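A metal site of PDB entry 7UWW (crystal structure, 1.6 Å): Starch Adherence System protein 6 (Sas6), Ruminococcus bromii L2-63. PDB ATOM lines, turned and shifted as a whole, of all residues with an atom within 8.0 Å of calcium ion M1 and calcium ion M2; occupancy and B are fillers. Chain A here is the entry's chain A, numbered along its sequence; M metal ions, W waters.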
ATOM      1  N   PRO A 250       4.313 -21.211  13.997  1.00  0.00           N
ATOM      2  CA  PRO A 250       4.649 -21.582  12.607  1.00  0.00           C
ATOM      3  C   PRO A 250       3.696 -22.571  11.963  1.00  0.00           C
ATOM      4  O   PRO A 250       3.550 -22.561  10.733  1.00  0.00           O
ATOM      5  CB  PRO A 250       6.060 -22.181  12.728  1.00  0.00           C
ATOM      6  CG  PRO A 250       6.692 -21.431  13.931  1.00  0.00           C
ATOM      7  CD  PRO A 250       5.479 -21.330  14.920  1.00  0.00           C
ATOM      8  N   GLY A 353      18.731 -27.140  14.873  1.00  0.00           N
ATOM      9  CA  GLY A 353      17.960 -25.958  15.187  1.00  0.00           C
ATOM     10  C   GLY A 353      18.422 -25.276  16.454  1.00  0.00           C
ATOM     11  O   GLY A 353      18.907 -25.918  17.398  1.00  0.00           O
ATOM     12  N   GLY A 354      18.252 -23.959  16.470  1.00  0.00           N
ATOM     13  CA  GLY A 354      18.528 -23.155  17.641  1.00  0.00           C
ATOM     14  C   GLY A 354      18.220 -21.716  17.324  1.00  0.00           C
ATOM     15  O   GLY A 354      17.790 -21.364  16.209  1.00  0.00           O
ATOM     16  N   THR A 355      18.429 -20.857  18.322  1.00  0.00           N
ATOM     17  CA  THR A 355      18.183 -19.428  18.171  1.00  0.00           C
ATOM     18  C   THR A 355      19.454 -18.701  18.565  1.00  0.00           C
ATOM     19  O   THR A 355      19.942 -18.894  19.693  1.00  0.00           O
ATOM     20  CB  THR A 355      17.015 -18.983  19.066  1.00  0.00           C
ATOM     21  OG1 THR A 355      15.826 -19.763  18.786  1.00  0.00           O
ATOM     22  CG2 THR A 355      16.738 -17.488  18.864  1.00  0.00           C
ATOM     23  N   LEU A 492      10.147 -19.708  22.997  1.00  0.00           N
ATOM     24  CA  LEU A 492       9.513 -21.017  22.981  1.00  0.00           C
ATOM     25  C   LEU A 492      10.109 -21.825  21.833  1.00  0.00           C
ATOM     26  O   LEU A 492      10.383 -21.290  20.752  1.00  0.00           O
ATOM     27  CB  LEU A 492       8.002 -20.913  22.778  1.00  0.00           C
ATOM     28  CG  LEU A 492       7.140 -20.225  23.810  1.00  0.00           C
ATOM     29  CD1 LEU A 492       5.690 -20.422  23.458  1.00  0.00           C
ATOM     30  CD2 LEU A 492       7.470 -20.776  25.167  1.00  0.00           C
ATOM     31  N   THR A 493      10.319 -23.120  22.093  1.00  0.00           N
ATOM     32  CA  THR A 493      10.789 -24.073  21.094  1.00  0.00           C
ATOM     33  C   THR A 493       9.804 -25.246  20.978  1.00  0.00           C
ATOM     34  O   THR A 493       8.850 -25.374  21.757  1.00  0.00           O
ATOM     35  CB  THR A 493      12.176 -24.629  21.464  1.00  0.00           C
ATOM     36  OG1 THR A 493      11.997 -25.664  22.454  1.00  0.00           O
ATOM     37  CG2 THR A 493      13.139 -23.516  21.926  1.00  0.00           C
ATOM     38  N   TYR A 494      10.066 -26.104  19.997  1.00  0.00           N
ATOM     39  CA  TYR A 494       9.491 -27.434  19.994  1.00  0.00           C
ATOM     40  C   TYR A 494      10.609 -28.461  20.083  1.00  0.00           C
ATOM     41  O   TYR A 494      10.604 -29.498  19.409  1.00  0.00           O
ATOM     42  CB  TYR A 494       8.617 -27.668  18.769  1.00  0.00           C
ATOM     43  CG  TYR A 494       7.618 -28.803  18.881  1.00  0.00           C
ATOM     44  CD1 TYR A 494       7.641 -29.678  19.935  1.00  0.00           C
ATOM     45  CD2 TYR A 494       6.670 -28.994  17.895  1.00  0.00           C
ATOM     46  CE1 TYR A 494       6.740 -30.725  20.030  1.00  0.00           C
ATOM     47  CE2 TYR A 494       5.749 -30.043  17.975  1.00  0.00           C
ATOM     48  CZ  TYR A 494       5.791 -30.910  19.052  1.00  0.00           C
ATOM     49  OH  TYR A 494       4.884 -31.969  19.142  1.00  0.00           O
ATOM     50  N   THR A 496      14.255 -27.652  19.869  1.00  0.00           N
ATOM     51  CA  THR A 496      15.535 -27.087  19.479  1.00  0.00           C
ATOM     52  C   THR A 496      15.371 -25.636  18.996  1.00  0.00           C
ATOM     53  O   THR A 496      15.593 -24.682  19.758  1.00  0.00           O
ATOM     54  CB  THR A 496      16.181 -27.937  18.381  1.00  0.00           C
ATOM     55  OG1 THR A 496      15.240 -28.173  17.317  1.00  0.00           O
ATOM     56  CG2 THR A 496      16.661 -29.260  18.971  1.00  0.00           C
ATOM     57  N   SER A 497      14.923 -25.484  17.746  1.00  0.00           N
ATOM     58  CA  SER A 497      14.697 -24.168  17.136  1.00  0.00           C
ATOM     59  C   SER A 497      13.582 -23.403  17.819  1.00  0.00           C
ATOM     60  O   SER A 497      12.612 -23.974  18.336  1.00  0.00           O
ATOM     61  CB  SER A 497      14.358 -24.334  15.646  1.00  0.00           C
ATOM     62  OG  SER A 497      14.408 -23.065  14.986  1.00  0.00           O
ATOM     63  N   GLY A 498      13.666 -22.088  17.738  1.00  0.00           N
ATOM     64  CA  GLY A 498      12.560 -21.263  18.197  1.00  0.00           C
ATOM     65  C   GLY A 498      11.333 -21.443  17.334  1.00  0.00           C
ATOM     66  O   GLY A 498      11.423 -21.805  16.161  1.00  0.00           O
ATOM     67  N   MET A 499      10.182 -21.252  17.966  1.00  0.00           N
ATOM     68  CA  MET A 499       8.857 -21.247  17.337  1.00  0.00           C
ATOM     69  C   MET A 499       8.113 -19.939  17.507  1.00  0.00           C
ATOM     70  O   MET A 499       7.400 -19.513  16.606  1.00  0.00           O
ATOM     71  CB  MET A 499       8.041 -22.376  17.949  1.00  0.00           C
ATOM     72  CG  MET A 499       8.611 -23.764  17.690  1.00  0.00           C
ATOM     73  SD  MET A 499       8.489 -24.274  15.975  1.00  0.00           S
ATOM     74  CE  MET A 499       6.792 -24.910  15.990  1.00  0.00           C
ATOM     75  N   ASP A 500       8.246 -19.288  18.658  1.00  0.00           N
ATOM     76  CA  ASP A 500       7.558 -18.043  18.993  1.00  0.00           C
ATOM     77  C   ASP A 500       8.429 -17.355  20.040  1.00  0.00           C
ATOM     78  O   ASP A 500       9.131 -18.028  20.789  1.00  0.00           O
ATOM     79  CB  ASP A 500       6.113 -18.349  19.481  1.00  0.00           C
ATOM     80  CG  ASP A 500       5.183 -17.147  19.430  1.00  0.00           C
ATOM     81  OD1 ASP A 500       5.644 -16.017  19.192  1.00  0.00           O
ATOM     82  OD2 ASP A 500       3.949 -17.327  19.662  1.00  0.00           O
ATOM     83  N   ASP A 505       9.755 -11.931  17.106  1.00  0.00           N
ATOM     84  CA  ASP A 505      10.824 -11.713  16.139  1.00  0.00           C
ATOM     85  C   ASP A 505      10.505 -12.400  14.817  1.00  0.00           C
ATOM     86  O   ASP A 505       9.985 -13.526  14.794  1.00  0.00           O
ATOM     87  CB  ASP A 505      12.155 -12.259  16.688  1.00  0.00           C
ATOM     88  CG  ASP A 505      13.328 -11.917  15.815  1.00  0.00           C
ATOM     89  OD1 ASP A 505      13.513 -12.546  14.747  1.00  0.00           O
ATOM     90  OD2 ASP A 505      14.066 -10.955  16.154  1.00  0.00           O
ATOM     91  N   PRO A 506      10.730 -11.719  13.688  1.00  0.00           N
ATOM     92  CA  PRO A 506      10.331 -12.300  12.387  1.00  0.00           C
ATOM     93  C   PRO A 506      11.095 -13.559  12.027  1.00  0.00           C
ATOM     94  O   PRO A 506      10.645 -14.303  11.138  1.00  0.00           O
ATOM     95  CB  PRO A 506      10.597 -11.149  11.383  1.00  0.00           C
ATOM     96  CG  PRO A 506      11.667 -10.343  12.016  1.00  0.00           C
ATOM     97  CD  PRO A 506      11.350 -10.383  13.522  1.00  0.00           C
ATOM     98  N   SER A 507      12.240 -13.843  12.666  1.00  0.00           N
ATOM     99  CA  SER A 507      12.912 -15.079  12.346  1.00  0.00           C
ATOM    100  C   SER A 507      12.105 -16.282  12.826  1.00  0.00           C
ATOM    101  O   SER A 507      12.428 -17.399  12.467  1.00  0.00           O
ATOM    102  CB  SER A 507      14.342 -15.129  12.915  1.00  0.00           C
ATOM    103  OG  SER A 507      14.348 -15.151  14.323  1.00  0.00           O
ATOM    104  N   MET A 508      11.042 -16.068  13.618  1.00  0.00           N
ATOM    105  CA  MET A 508      10.234 -17.213  14.034  1.00  0.00           C
ATOM    106  C   MET A 508       9.360 -17.727  12.878  1.00  0.00           C
ATOM    107  O   MET A 508       8.859 -18.856  12.948  1.00  0.00           O
ATOM    108  CB  MET A 508       9.361 -16.853  15.229  1.00  0.00           C
ATOM    109  CG  MET A 508      10.080 -16.522  16.518  1.00  0.00           C
ATOM    110  SD  MET A 508      11.068 -17.880  17.094  1.00  0.00           S
ATOM    111  CE  MET A 508      12.695 -17.224  16.769  1.00  0.00           C
ATOM    112  N   LEU A 509       9.177 -16.918  11.852  1.00  0.00           N
ATOM    113  CA  LEU A 509       8.247 -17.211  10.755  1.00  0.00           C
ATOM    114  C   LEU A 509       8.879 -17.096   9.369  1.00  0.00           C
ATOM    115  O   LEU A 509       8.178 -17.308   8.383  1.00  0.00           O
ATOM    116  CB  LEU A 509       7.045 -16.282  10.841  1.00  0.00           C
ATOM    117  CG  LEU A 509       6.160 -16.506  12.105  1.00  0.00           C
ATOM    118  CD1 LEU A 509       5.061 -15.441  12.129  1.00  0.00           C
ATOM    119  CD2 LEU A 509       5.562 -17.857  12.137  1.00  0.00           C
ATOM    120  N   ASP A 510      10.174 -16.785   9.280  1.00  0.00           N
ATOM    121  CA  ASP A 510      10.789 -16.550   7.980  1.00  0.00           C
ATOM    122  C   ASP A 510      10.802 -17.794   7.107  1.00  0.00           C
ATOM    123  O   ASP A 510      10.835 -17.662   5.877  1.00  0.00           O
ATOM    124  CB  ASP A 510      12.189 -15.929   8.152  1.00  0.00           C
ATOM    125  CG  ASP A 510      13.217 -16.851   8.841  1.00  0.00           C
ATOM    126  OD1 ASP A 510      12.863 -17.827   9.510  1.00  0.00           O
ATOM    127  OD2 ASP A 510      14.425 -16.557   8.723  1.00  0.00           O
ATOM    128  N   GLN A 511      10.701 -19.000   7.701  1.00  0.00           N
ATOM    129  CA  GLN A 511      10.652 -20.281   6.990  1.00  0.00           C
ATOM    130  C   GLN A 511       9.471 -21.130   7.461  1.00  0.00           C
ATOM    131  O   GLN A 511       9.516 -22.370   7.380  1.00  0.00           O
ATOM    132  CB  GLN A 511      11.963 -21.027   7.156  1.00  0.00           C
ATOM    133  CG  GLN A 511      13.160 -20.165   6.715  1.00  0.00           C
ATOM    134  CD  GLN A 511      14.432 -20.963   6.491  1.00  0.00           C
ATOM    135  OE1 GLN A 511      14.889 -21.108   5.375  1.00  0.00           O
ATOM    136  NE2 GLN A 511      15.021 -21.463   7.567  1.00  0.00           N
ATOM    137  N   ALA A 512       8.384 -20.489   7.891  1.00  0.00           N
ATOM    138  CA  ALA A 512       7.281 -21.223   8.507  1.00  0.00           C
ATOM    139  C   ALA A 512       6.547 -22.115   7.505  1.00  0.00           C
ATOM    140  O   ALA A 512       6.051 -23.191   7.871  1.00  0.00           O
ATOM    141  CB  ALA A 512       6.284 -20.262   9.127  1.00  0.00           C
ATOM    142  N   SER A 523       6.166 -27.838  10.051  1.00  0.00           N
ATOM    143  CA  SER A 523       6.950 -26.661   9.683  1.00  0.00           C
ATOM    144  C   SER A 523       8.434 -26.844   9.973  1.00  0.00           C
ATOM    145  O   SER A 523       8.809 -27.343  11.043  1.00  0.00           O
ATOM    146  CB  SER A 523       6.456 -25.420  10.428  1.00  0.00           C
ATOM    147  OG  SER A 523       7.241 -24.295  10.109  1.00  0.00           O
ATOM    148  N   HIS A 524       9.257 -26.430   8.996  1.00  0.00           N
ATOM    149  CA  HIS A 524      10.700 -26.357   9.088  1.00  0.00           C
ATOM    150  C   HIS A 524      11.175 -25.434  10.203  1.00  0.00           C
ATOM    151  O   HIS A 524      12.334 -25.531  10.616  1.00  0.00           O
ATOM    152  CB  HIS A 524      11.231 -25.870   7.732  1.00  0.00           C
ATOM    153  CG  HIS A 524      12.722 -25.790   7.632  1.00  0.00           C
ATOM    154  ND1 HIS A 524      13.530 -26.880   7.816  1.00  0.00           N
ATOM    155  CD2 HIS A 524      13.544 -24.748   7.340  1.00  0.00           C
ATOM    156  CE1 HIS A 524      14.800 -26.526   7.643  1.00  0.00           C
ATOM    157  NE2 HIS A 524      14.835 -25.230   7.368  1.00  0.00           N
ATOM    158  N   GLU A 525      10.309 -24.567  10.716  1.00  0.00           N
ATOM    159  CA  GLU A 525      10.699 -23.691  11.810  1.00  0.00           C
ATOM    160  C   GLU A 525      11.053 -24.466  13.068  1.00  0.00           C
ATOM    161  O   GLU A 525      11.660 -23.899  13.975  1.00  0.00           O
ATOM    162  CB  GLU A 525       9.570 -22.688  12.130  1.00  0.00           C
ATOM    163  CG  GLU A 525       9.570 -21.454  11.239  1.00  0.00           C
ATOM    164  CD  GLU A 525      10.825 -20.578  11.391  1.00  0.00           C
ATOM    165  OE1 GLU A 525      11.561 -20.775  12.408  1.00  0.00           O
ATOM    166  OE2 GLU A 525      11.046 -19.718  10.493  1.00  0.00           O
ATOM    167  N   LYS A 526      10.654 -25.733  13.154  1.00  0.00           N
ATOM    168  CA  LYS A 526      11.022 -26.565  14.293  1.00  0.00           C
ATOM    169  C   LYS A 526      12.505 -26.923  14.322  1.00  0.00           C
ATOM    170  O   LYS A 526      12.998 -27.325  15.373  1.00  0.00           O
ATOM    171  CB  LYS A 526      10.197 -27.875  14.253  1.00  0.00           C
ATOM    172  CG  LYS A 526       8.717 -27.686  14.403  1.00  0.00           C
ATOM    173  CD  LYS A 526       7.998 -29.023  14.550  1.00  0.00           C
ATOM    174  CE  LYS A 526       7.941 -29.804  13.233  1.00  0.00           C
ATOM    175  NZ  LYS A 526       7.099 -31.076  13.385  1.00  0.00           N
ATOM    176  N   GLU A 527      13.210 -26.763  13.202  1.00  0.00           N
ATOM    177  CA  GLU A 527      14.569 -27.253  13.077  1.00  0.00           C
ATOM    178  C   GLU A 527      15.551 -26.278  12.431  1.00  0.00           C
ATOM    179  O   GLU A 527      16.714 -26.647  12.247  1.00  0.00           O
ATOM    180  CB  GLU A 527      14.551 -28.565  12.246  1.00  0.00           C
ATOM    181  CG  GLU A 527      14.294 -28.307  10.749  1.00  0.00           C
ATOM    182  CD  GLU A 527      14.107 -29.583   9.921  1.00  0.00           C
ATOM    183  OE1 GLU A 527      14.618 -30.670  10.329  1.00  0.00           O
ATOM    184  OE2 GLU A 527      13.475 -29.477   8.840  1.00  0.00           O
ATOM    185  N   ASP A 528      15.154 -25.048  12.119  1.00  0.00           N
ATOM    186  CA  ASP A 528      16.049 -24.142  11.431  1.00  0.00           C
ATOM    187  C   ASP A 528      16.825 -23.292  12.433  1.00  0.00           C
ATOM    188  O   ASP A 528      16.671 -23.417  13.646  1.00  0.00           O
ATOM    189  CB  ASP A 528      15.296 -23.261  10.429  1.00  0.00           C
ATOM    190  CG  ASP A 528      14.330 -22.296  11.089  1.00  0.00           C
ATOM    191  OD1 ASP A 528      13.832 -22.610  12.195  1.00  0.00           O
ATOM    192  OD2 ASP A 528      13.995 -21.250  10.473  1.00  0.00           O
ATOM    193  N   ILE A 529      17.677 -22.410  11.912  1.00  0.00           N
ATOM    194  CA  ILE A 529      18.464 -21.506  12.743  1.00  0.00           C
ATOM    195  C   ILE A 529      17.843 -20.124  12.677  1.00  0.00           C
ATOM    196  O   ILE A 529      17.732 -19.510  11.614  1.00  0.00           O
ATOM    197  CB  ILE A 529      19.942 -21.503  12.312  1.00  0.00           C
ATOM    198  CG1 ILE A 529      20.563 -22.879  12.572  1.00  0.00           C
ATOM    199  CG2 ILE A 529      20.739 -20.424  13.098  1.00  0.00           C
ATOM    200  CD1 ILE A 529      22.063 -22.944  12.290  1.00  0.00           C
ATOM    201  N   ASP A 530      17.362 -19.656  13.823  1.00  0.00           N
ATOM    202  CA  ASP A 530      16.702 -18.378  13.981  1.00  0.00           C
ATOM    203  C   ASP A 530      17.776 -17.420  14.473  1.00  0.00           C
ATOM    204  O   ASP A 530      18.804 -17.865  14.980  1.00  0.00           O
ATOM    205  CB  ASP A 530      15.536 -18.463  14.960  1.00  0.00           C
ATOM    206  CG  ASP A 530      14.472 -19.506  14.554  1.00  0.00           C
ATOM    207  OD1 ASP A 530      14.239 -19.717  13.337  1.00  0.00           O
ATOM    208  OD2 ASP A 530      13.884 -20.152  15.479  1.00  0.00           O
ATOM    209  N   ASN A 531      17.552 -16.133  14.291  1.00  0.00           N
ATOM    210  CA  ASN A 531      18.524 -15.148  14.756  1.00  0.00           C
ATOM    211  C   ASN A 531      17.784 -13.874  15.136  1.00  0.00           C
ATOM    212  O   ASN A 531      17.118 -13.261  14.312  1.00  0.00           O
ATOM    213  CB  ASN A 531      19.579 -14.856  13.699  1.00  0.00           C
ATOM    214  CG  ASN A 531      20.659 -13.921  14.220  1.00  0.00           C
ATOM    215  OD1 ASN A 531      20.509 -12.712  14.179  1.00  0.00           O
ATOM    216  ND2 ASN A 531      21.743 -14.492  14.763  1.00  0.00           N
HETATM  217 CA    CA M   1      12.673 -21.674  14.120  1.00  0.00          CA
HETATM  218 CA    CA M   2      13.263 -19.202  11.278  1.00  0.00          CA
HETATM  219  O   HOH W   1      15.356 -18.248  10.590  1.00  0.00           O
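The backbone NH (N) of Gln 511 lies close to the side-chain carboxylate (OE2) of Glu 525.
The backbone NH of Glu 525 sits close to the side-chain hydroxyl of Ser 523.
The side-chain hydroxyl of Ser 507 lies within hydrogen-bond range of the backbone NH of Asn 531 (3.4 Å).
The side-chain carboxylate of Asp 505 is in hydrogen-bond range of the backbone NH of Ser 507 (2.8 Å).
The side-chain amide nitrogen (NE2) of Gln 511 lies close to the side-chain carboxylate (OD2) of Asp 528 (3.1 Å).
O of Asp 528 lies within hydrogen-bond range of N of Gly 354 (3.3 Å).
The backbone carbonyl oxygen (O) of Gly 354 sits at hydrogen-bond distance from the backbone NH (N) of Asp 530, at 3.0 Å.
N of Gly 498 lies within hydrogen-bond range of OG1 of Thr 355, 3.3 Å away.
Of the 29 residues printed, 5 come within 4 Å of calcium ion M1.
The nearest printed residue that does not touch calcium ion M1 is Ser 507 (4.6 Å).
Of the 29 residues printed, 5 come within 4 Å of calcium ion M2.
Along chain A the residues within 4 Å of calcium ion M2 span positions 507 to 530.
Calcium ion M1 is bound by the side-chain carboxylate (OE1) of Glu 525 (2.2 Å), the side-chain carboxylate (OD2) of Asp 530 (2.4 Å), the side-chain hydroxyl (OG) of Ser 497 (2.4 Å), the backbone carbonyl oxygen (O) of Gly 498 (2.4 Å), the side-chain carboxylate (OD1) of Asp 528 (2.4 Å), the backbone carbonyl oxygen (O) of Glu 525 (2.4 Å) and the side-chain carboxylate (OD1) of Asp 530 (2.6 Å).
Calcium ion M1 has seven donor atoms within binding distance.
Calcium ion M2 is bound by OD1 of Asp 510 (2.3 Å), O of Ser 507 (2.3 Å), OD2 of Asp 528 (2.3 Å), OD1 of Asp 530 (2.3 Å), water W1 (2.4 Å), OE2 of Glu 525 (2.4 Å) and OE1 of Glu 525 (2.6 Å).
Calcium ion M2 has seven donor atoms within binding distance.
Water W1 bridges the side-chain carboxylate (OD2) of Asp 510 (2.7 Å) and the backbone carbonyl oxygen (O) of Ile 529 (2.9 Å).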
